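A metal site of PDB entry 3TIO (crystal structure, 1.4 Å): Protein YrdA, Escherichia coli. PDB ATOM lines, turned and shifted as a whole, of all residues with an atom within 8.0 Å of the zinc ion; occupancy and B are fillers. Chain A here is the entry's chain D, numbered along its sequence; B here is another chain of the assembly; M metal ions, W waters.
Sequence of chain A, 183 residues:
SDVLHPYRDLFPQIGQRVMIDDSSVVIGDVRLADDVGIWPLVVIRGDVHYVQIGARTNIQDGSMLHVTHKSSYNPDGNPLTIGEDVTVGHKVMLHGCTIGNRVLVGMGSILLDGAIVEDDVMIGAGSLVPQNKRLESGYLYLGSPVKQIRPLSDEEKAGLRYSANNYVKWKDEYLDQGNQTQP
OD1 of Asp 113 lies within hydrogen-bond range of ND1 of His 95 (2.8 Å). The backbone NH (N) of His 90 of chain B lies close to the side-chain amide oxygen (OE1) of Gln 60 of chain B, 3.3 Å away. A ring nitrogen (ND1) of His 90 of chain B lies within hydrogen-bond range of the side-chain carboxylate of Asp 61 of chain B. A ring nitrogen (ND1) of His 90 of chain B is in hydrogen-bond range of the side-chain sulfur (SD) of Met 64. A ring nitrogen (NE2) of His 66 is in hydrogen-bond range of the guanidinium group (NH1) of Arg 45 (3.2 Å). The backbone NH (N) of His 66 lies within hydrogen-bond range of the backbone carbonyl oxygen (O) of Leu 94, at 3.0 Å. The backbone NH (N) of Gly 96 lies within hydrogen-bond range of the backbone carbonyl oxygen (O) of His 66, at 3.0 Å. OD2 of Asp 47 sits at hydrogen-bond distance from NE2 of His 66, at 3.1 Å.
O of Val 67 touches the zinc ion, at 3.8 Å. The nearest printed residue that does not touch the zinc ion is Tyr 167 of chain B (4.03 Å).
A ring nitrogen (NE2) of His 95 binds the zinc ion, 2.1 Å away. A ring nitrogen (NE2) of His 90 of chain B binds the zinc ion (2.1 Å). ND1 of His 66 binds the zinc ion (2.1 Å). Water W1 binds the zinc ion.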
ATOM      1  N   ARG A  45     -10.254   6.482  27.275  1.00  0.00           N
ATOM      2  CA  ARG A  45     -10.287   6.399  25.820  1.00  0.00           C
ATOM      3  C   ARG A  45      -9.796   5.058  25.297  1.00  0.00           C
ATOM      4  O   ARG A  45      -8.602   4.794  25.239  1.00  0.00           O
ATOM      5  CB  ARG A  45      -9.454   7.561  25.235  1.00  0.00           C
ATOM      6  CG  ARG A  45      -9.513   7.713  23.714  1.00  0.00           C
ATOM      7  CD  ARG A  45      -9.370   9.169  23.268  1.00  0.00           C
ATOM      8  NE  ARG A  45      -8.076   9.784  23.557  1.00  0.00           N
ATOM      9  CZ  ARG A  45      -6.980   9.649  22.814  1.00  0.00           C
ATOM     10  NH1 ARG A  45      -7.009   8.909  21.711  1.00  0.00           N
ATOM     11  NH2 ARG A  45      -5.859  10.270  23.164  1.00  0.00           N
ATOM     12  N   ASP A  47     -10.038   3.763  22.177  1.00  0.00           N
ATOM     13  CA  ASP A  47     -10.218   3.821  20.737  1.00  0.00           C
ATOM     14  C   ASP A  47      -9.293   2.920  19.931  1.00  0.00           C
ATOM     15  O   ASP A  47      -9.771   2.054  19.195  1.00  0.00           O
ATOM     16  CB  ASP A  47     -10.147   5.287  20.231  1.00  0.00           C
ATOM     17  CG  ASP A  47      -8.960   6.066  20.765  1.00  0.00           C
ATOM     18  OD1 ASP A  47      -8.942   7.301  20.534  1.00  0.00           O
ATOM     19  OD2 ASP A  47      -8.054   5.484  21.405  1.00  0.00           O
ATOM     20  N   VAL A  48      -7.981   3.094  20.071  1.00  0.00           N
ATOM     21  CA  VAL A  48      -7.033   2.269  19.314  1.00  0.00           C
ATOM     22  C   VAL A  48      -6.799   0.896  19.933  1.00  0.00           C
ATOM     23  O   VAL A  48      -6.134   0.041  19.333  1.00  0.00           O
ATOM     24  CB  VAL A  48      -5.685   3.000  19.126  1.00  0.00           C
ATOM     25  CG1 VAL A  48      -5.916   4.278  18.336  1.00  0.00           C
ATOM     26  CG2 VAL A  48      -5.052   3.307  20.470  1.00  0.00           C
ATOM     27  N   MET A  64      -6.751   9.724  33.895  1.00  0.00           N
ATOM     28  CA  MET A  64      -6.723   9.665  32.446  1.00  0.00           C
ATOM     29  C   MET A  64      -6.243   8.270  32.089  1.00  0.00           C
ATOM     30  O   MET A  64      -5.136   7.874  32.473  1.00  0.00           O
ATOM     31  CB  MET A  64      -5.765  10.724  31.895  1.00  0.00           C
ATOM     32  CG  MET A  64      -6.061  11.180  30.465  1.00  0.00           C
ATOM     33  SD  MET A  64      -5.625   9.971  29.209  1.00  0.00           S
ATOM     34  CE  MET A  64      -7.208   9.646  28.434  1.00  0.00           C
ATOM     35  N   LEU A  65      -7.088   7.534  31.375  1.00  0.00           N
ATOM     36  CA  LEU A  65      -6.782   6.159  30.965  1.00  0.00           C
ATOM     37  C   LEU A  65      -6.715   6.013  29.448  1.00  0.00           C
ATOM     38  O   LEU A  65      -7.673   6.322  28.748  1.00  0.00           O
ATOM     39  CB  LEU A  65      -7.869   5.210  31.519  1.00  0.00           C
ATOM     40  CG  LEU A  65      -7.819   4.796  32.995  1.00  0.00           C
ATOM     41  CD1 LEU A  65      -7.796   6.012  33.909  1.00  0.00           C
ATOM     42  CD2 LEU A  65      -9.019   3.903  33.305  1.00  0.00           C
ATOM     43  N   HIS A  66      -5.564   5.574  28.942  1.00  0.00           N
ATOM     44  CA  HIS A  66      -5.431   5.356  27.508  1.00  0.00           C
ATOM     45  C   HIS A  66      -4.651   4.092  27.226  1.00  0.00           C
ATOM     46  O   HIS A  66      -4.252   3.370  28.150  1.00  0.00           O
ATOM     47  CB  HIS A  66      -4.791   6.548  26.794  1.00  0.00           C
ATOM     48  CG  HIS A  66      -5.027   6.551  25.317  1.00  0.00           C
ATOM     49  ND1 HIS A  66      -4.087   6.996  24.409  1.00  0.00           N
ATOM     50  CD2 HIS A  66      -6.095   6.151  24.582  1.00  0.00           C
ATOM     51  CE1 HIS A  66      -4.572   6.875  23.183  1.00  0.00           C
ATOM     52  NE2 HIS A  66      -5.783   6.366  23.259  1.00  0.00           N
ATOM     53  N   VAL A  67      -4.428   3.836  25.947  1.00  0.00           N
ATOM     54  CA  VAL A  67      -3.760   2.629  25.469  1.00  0.00           C
ATOM     55  C   VAL A  67      -2.843   2.916  24.284  1.00  0.00           C
ATOM     56  O   VAL A  67      -2.870   4.012  23.733  1.00  0.00           O
ATOM     57  CB  VAL A  67      -4.839   1.618  25.000  1.00  0.00           C
ATOM     58  CG1 VAL A  67      -5.687   1.164  26.179  1.00  0.00           C
ATOM     59  CG2 VAL A  67      -5.741   2.294  23.955  1.00  0.00           C
ATOM     60  N   THR A  68      -2.051   1.930  23.899  1.00  0.00           N
ATOM     61  CA  THR A  68      -1.162   2.073  22.757  1.00  0.00           C
ATOM     62  C   THR A  68      -1.651   1.156  21.632  1.00  0.00           C
ATOM     63  O   THR A  68      -1.920  -0.024  21.852  1.00  0.00           O
ATOM     64  CB  THR A  68       0.296   1.738  23.104  1.00  0.00           C
ATOM     65  OG1 THR A  68       0.824   2.751  23.974  1.00  0.00           O
ATOM     66  CG2 THR A  68       1.152   1.670  21.850  1.00  0.00           C
ATOM     67  N   HIS A  69      -1.759   1.716  20.432  1.00  0.00           N
ATOM     68  CA  HIS A  69      -2.242   0.987  19.266  1.00  0.00           C
ATOM     69  C   HIS A  69      -1.324  -0.154  18.826  1.00  0.00           C
ATOM     70  O   HIS A  69      -0.155  -0.205  19.194  1.00  0.00           O
ATOM     71  CB  HIS A  69      -2.440   1.938  18.088  1.00  0.00           C
ATOM     72  CG  HIS A  69      -1.154   2.397  17.456  1.00  0.00           C
ATOM     73  ND1 HIS A  69      -0.187   3.094  18.152  1.00  0.00           N
ATOM     74  CD2 HIS A  69      -0.678   2.232  16.202  1.00  0.00           C
ATOM     75  CE1 HIS A  69       0.825   3.343  17.337  1.00  0.00           C
ATOM     76  NE2 HIS A  69       0.557   2.833  16.158  1.00  0.00           N
ATOM     77  N   MET A  93      -2.581   8.560  35.978  1.00  0.00           N
ATOM     78  CA  MET A  93      -2.389   8.389  34.545  1.00  0.00           C
ATOM     79  C   MET A  93      -2.084   6.916  34.303  1.00  0.00           C
ATOM     80  O   MET A  93      -1.062   6.415  34.785  1.00  0.00           O
ATOM     81  CB  MET A  93      -1.211   9.239  34.078  1.00  0.00           C
ATOM     82  CG  MET A  93      -0.813   9.068  32.614  1.00  0.00           C
ATOM     83  SD  MET A  93      -1.962   9.858  31.461  1.00  0.00           S
ATOM     84  CE  MET A  93      -2.486   8.429  30.466  1.00  0.00           C
ATOM     85  N   LEU A  94      -2.974   6.218  33.613  1.00  0.00           N
ATOM     86  CA  LEU A  94      -2.773   4.802  33.311  1.00  0.00           C
ATOM     87  C   LEU A  94      -2.673   4.670  31.805  1.00  0.00           C
ATOM     88  O   LEU A  94      -3.566   5.088  31.082  1.00  0.00           O
ATOM     89  CB  LEU A  94      -3.946   3.948  33.814  1.00  0.00           C
ATOM     90  CG  LEU A  94      -4.239   3.952  35.315  1.00  0.00           C
ATOM     91  CD1 LEU A  94      -5.368   2.961  35.607  1.00  0.00           C
ATOM     92  CD2 LEU A  94      -2.991   3.557  36.096  1.00  0.00           C
ATOM     93  N   HIS A  95      -1.577   4.085  31.327  1.00  0.00           N
ATOM     94  CA  HIS A  95      -1.396   3.932  29.906  1.00  0.00           C
ATOM     95  C   HIS A  95      -0.947   2.542  29.521  1.00  0.00           C
ATOM     96  O   HIS A  95       0.190   2.154  29.793  1.00  0.00           O
ATOM     97  CB  HIS A  95      -0.384   4.968  29.399  1.00  0.00           C
ATOM     98  CG  HIS A  95      -0.576   5.349  27.965  1.00  0.00           C
ATOM     99  ND1 HIS A  95      -0.154   4.559  26.912  1.00  0.00           N
ATOM    100  CD2 HIS A  95      -1.186   6.415  27.409  1.00  0.00           C
ATOM    101  CE1 HIS A  95      -0.502   5.132  25.777  1.00  0.00           C
ATOM    102  NE2 HIS A  95      -1.125   6.261  26.052  1.00  0.00           N
ATOM    103  N   GLY A  96      -1.855   1.784  28.908  1.00  0.00           N
ATOM    104  CA  GLY A  96      -1.557   0.435  28.431  1.00  0.00           C
ATOM    105  C   GLY A  96      -0.893  -0.518  29.398  1.00  0.00           C
ATOM    106  O   GLY A  96      -0.040  -1.304  29.006  1.00  0.00           O
ATOM    107  N   ASP A 113       3.117   1.921  29.677  1.00  0.00           N
ATOM    108  CA  ASP A 113       2.845   0.755  28.847  1.00  0.00           C
ATOM    109  C   ASP A 113       3.606  -0.496  29.198  1.00  0.00           C
ATOM    110  O   ASP A 113       4.819  -0.479  29.410  1.00  0.00           O
ATOM    111  CB  ASP A 113       3.092   1.119  27.384  1.00  0.00           C
ATOM    112  CG  ASP A 113       2.233   2.279  26.937  1.00  0.00           C
ATOM    113  OD1 ASP A 113       1.074   2.048  26.541  1.00  0.00           O
ATOM    114  OD2 ASP A 113       2.709   3.425  27.018  1.00  0.00           O
ATOM    115  N   GLN B  60      -2.862  16.218  23.800  1.00  0.00           N
ATOM    116  CA  GLN B  60      -3.579  15.098  24.379  1.00  0.00           C
ATOM    117  C   GLN B  60      -4.383  15.353  25.640  1.00  0.00           C
ATOM    118  O   GLN B  60      -4.216  16.361  26.325  1.00  0.00           O
ATOM    119  CB  GLN B  60      -2.611  13.937  24.553  1.00  0.00           C
ATOM    120  CG  GLN B  60      -2.149  13.386  23.210  1.00  0.00           C
ATOM    121  CD  GLN B  60      -1.076  12.335  23.347  1.00  0.00           C
ATOM    122  OE1 GLN B  60      -1.078  11.552  24.294  1.00  0.00           O
ATOM    123  NE2 GLN B  60      -0.152  12.294  22.388  1.00  0.00           N
ATOM    124  N   ASP B  61      -5.267  14.396  25.910  1.00  0.00           N
ATOM    125  CA  ASP B  61      -6.212  14.410  27.026  1.00  0.00           C
ATOM    126  C   ASP B  61      -5.670  14.885  28.353  1.00  0.00           C
ATOM    127  O   ASP B  61      -4.626  14.423  28.812  1.00  0.00           O
ATOM    128  CB  ASP B  61      -6.800  13.011  27.261  1.00  0.00           C
ATOM    129  CG  ASP B  61      -6.975  12.204  25.986  1.00  0.00           C
ATOM    130  OD1 ASP B  61      -5.954  11.946  25.304  1.00  0.00           O
ATOM    131  OD2 ASP B  61      -8.117  11.808  25.675  1.00  0.00           O
ATOM    132  N   GLY B  89       1.873  15.009  25.120  1.00  0.00           N
ATOM    133  CA  GLY B  89       1.284  13.875  25.810  1.00  0.00           C
ATOM    134  C   GLY B  89       0.158  14.139  26.781  1.00  0.00           C
ATOM    135  O   GLY B  89      -0.075  15.267  27.196  1.00  0.00           O
ATOM    136  N   HIS B  90      -0.532  13.076  27.156  1.00  0.00           N
ATOM    137  CA  HIS B  90      -1.643  13.179  28.094  1.00  0.00           C
ATOM    138  C   HIS B  90      -1.213  13.892  29.369  1.00  0.00           C
ATOM    139  O   HIS B  90      -0.101  13.689  29.867  1.00  0.00           O
ATOM    140  CB  HIS B  90      -2.166  11.802  28.502  1.00  0.00           C
ATOM    141  CG  HIS B  90      -2.440  10.874  27.371  1.00  0.00           C
ATOM    142  ND1 HIS B  90      -3.547  10.988  26.549  1.00  0.00           N
ATOM    143  CD2 HIS B  90      -1.768   9.781  26.933  1.00  0.00           C
ATOM    144  CE1 HIS B  90      -3.541  10.004  25.669  1.00  0.00           C
ATOM    145  NE2 HIS B  90      -2.475   9.256  25.890  1.00  0.00           N
ATOM    146  N   MET B 107       3.902  12.110  28.523  1.00  0.00           N
ATOM    147  CA  MET B 107       2.733  12.300  29.364  1.00  0.00           C
ATOM    148  C   MET B 107       3.055  12.607  30.825  1.00  0.00           C
ATOM    149  O   MET B 107       3.979  12.045  31.410  1.00  0.00           O
ATOM    150  CB  MET B 107       1.821  11.070  29.267  1.00  0.00           C
ATOM    151  CG  MET B 107       2.399   9.797  29.891  1.00  0.00           C
ATOM    152  SD  MET B 107       1.350   8.343  29.575  1.00  0.00           S
ATOM    153  CE  MET B 107       2.028   7.771  28.035  1.00  0.00           C
ATOM    154  N   TYR B 167      -1.644  10.808  15.010  1.00  0.00           N
ATOM    155  CA  TYR B 167      -2.630  11.631  15.674  1.00  0.00           C
ATOM    156  C   TYR B 167      -3.453  12.479  14.717  1.00  0.00           C
ATOM    157  O   TYR B 167      -4.604  12.804  15.020  1.00  0.00           O
ATOM    158  CB  TYR B 167      -1.992  12.476  16.774  1.00  0.00           C
ATOM    159  CG  TYR B 167      -2.253  11.872  18.138  1.00  0.00           C
ATOM    160  CD1 TYR B 167      -1.341  10.980  18.714  1.00  0.00           C
ATOM    161  CD2 TYR B 167      -3.431  12.137  18.820  1.00  0.00           C
ATOM    162  CE1 TYR B 167      -1.631  10.352  19.924  1.00  0.00           C
ATOM    163  CE2 TYR B 167      -3.729  11.522  20.030  1.00  0.00           C
ATOM    164  CZ  TYR B 167      -2.826  10.631  20.578  1.00  0.00           C
ATOM    165  OH  TYR B 167      -3.128  10.021  21.775  1.00  0.00           O
ATOM    166  N   TRP B 170      -5.980  10.039  13.546  1.00  0.00           N
ATOM    167  CA  TRP B 170      -6.955   9.744  14.579  1.00  0.00           C
ATOM    168  C   TRP B 170      -7.937  10.889  14.807  1.00  0.00           C
ATOM    169  O   TRP B 170      -9.132  10.640  14.990  1.00  0.00           O
ATOM    170  CB  TRP B 170      -6.247   9.354  15.887  1.00  0.00           C
ATOM    171  CG  TRP B 170      -5.556   8.010  15.778  1.00  0.00           C
ATOM    172  CD1 TRP B 170      -5.960   6.946  15.029  1.00  0.00           C
ATOM    173  CD2 TRP B 170      -4.349   7.602  16.438  1.00  0.00           C
ATOM    174  NE1 TRP B 170      -5.079   5.896  15.192  1.00  0.00           N
ATOM    175  CE2 TRP B 170      -4.083   6.269  16.044  1.00  0.00           C
ATOM    176  CE3 TRP B 170      -3.464   8.233  17.327  1.00  0.00           C
ATOM    177  CZ2 TRP B 170      -2.967   5.550  16.504  1.00  0.00           C
ATOM    178  CZ3 TRP B 170      -2.353   7.511  17.796  1.00  0.00           C
ATOM    179  CH2 TRP B 170      -2.118   6.190  17.377  1.00  0.00           C
HETATM  180 ZN    ZN M   1      -2.117   7.550  24.794  1.00  0.00          ZN
HETATM  181  O   HOH W   1      -1.132   7.830  22.838  1.00  0.00           O
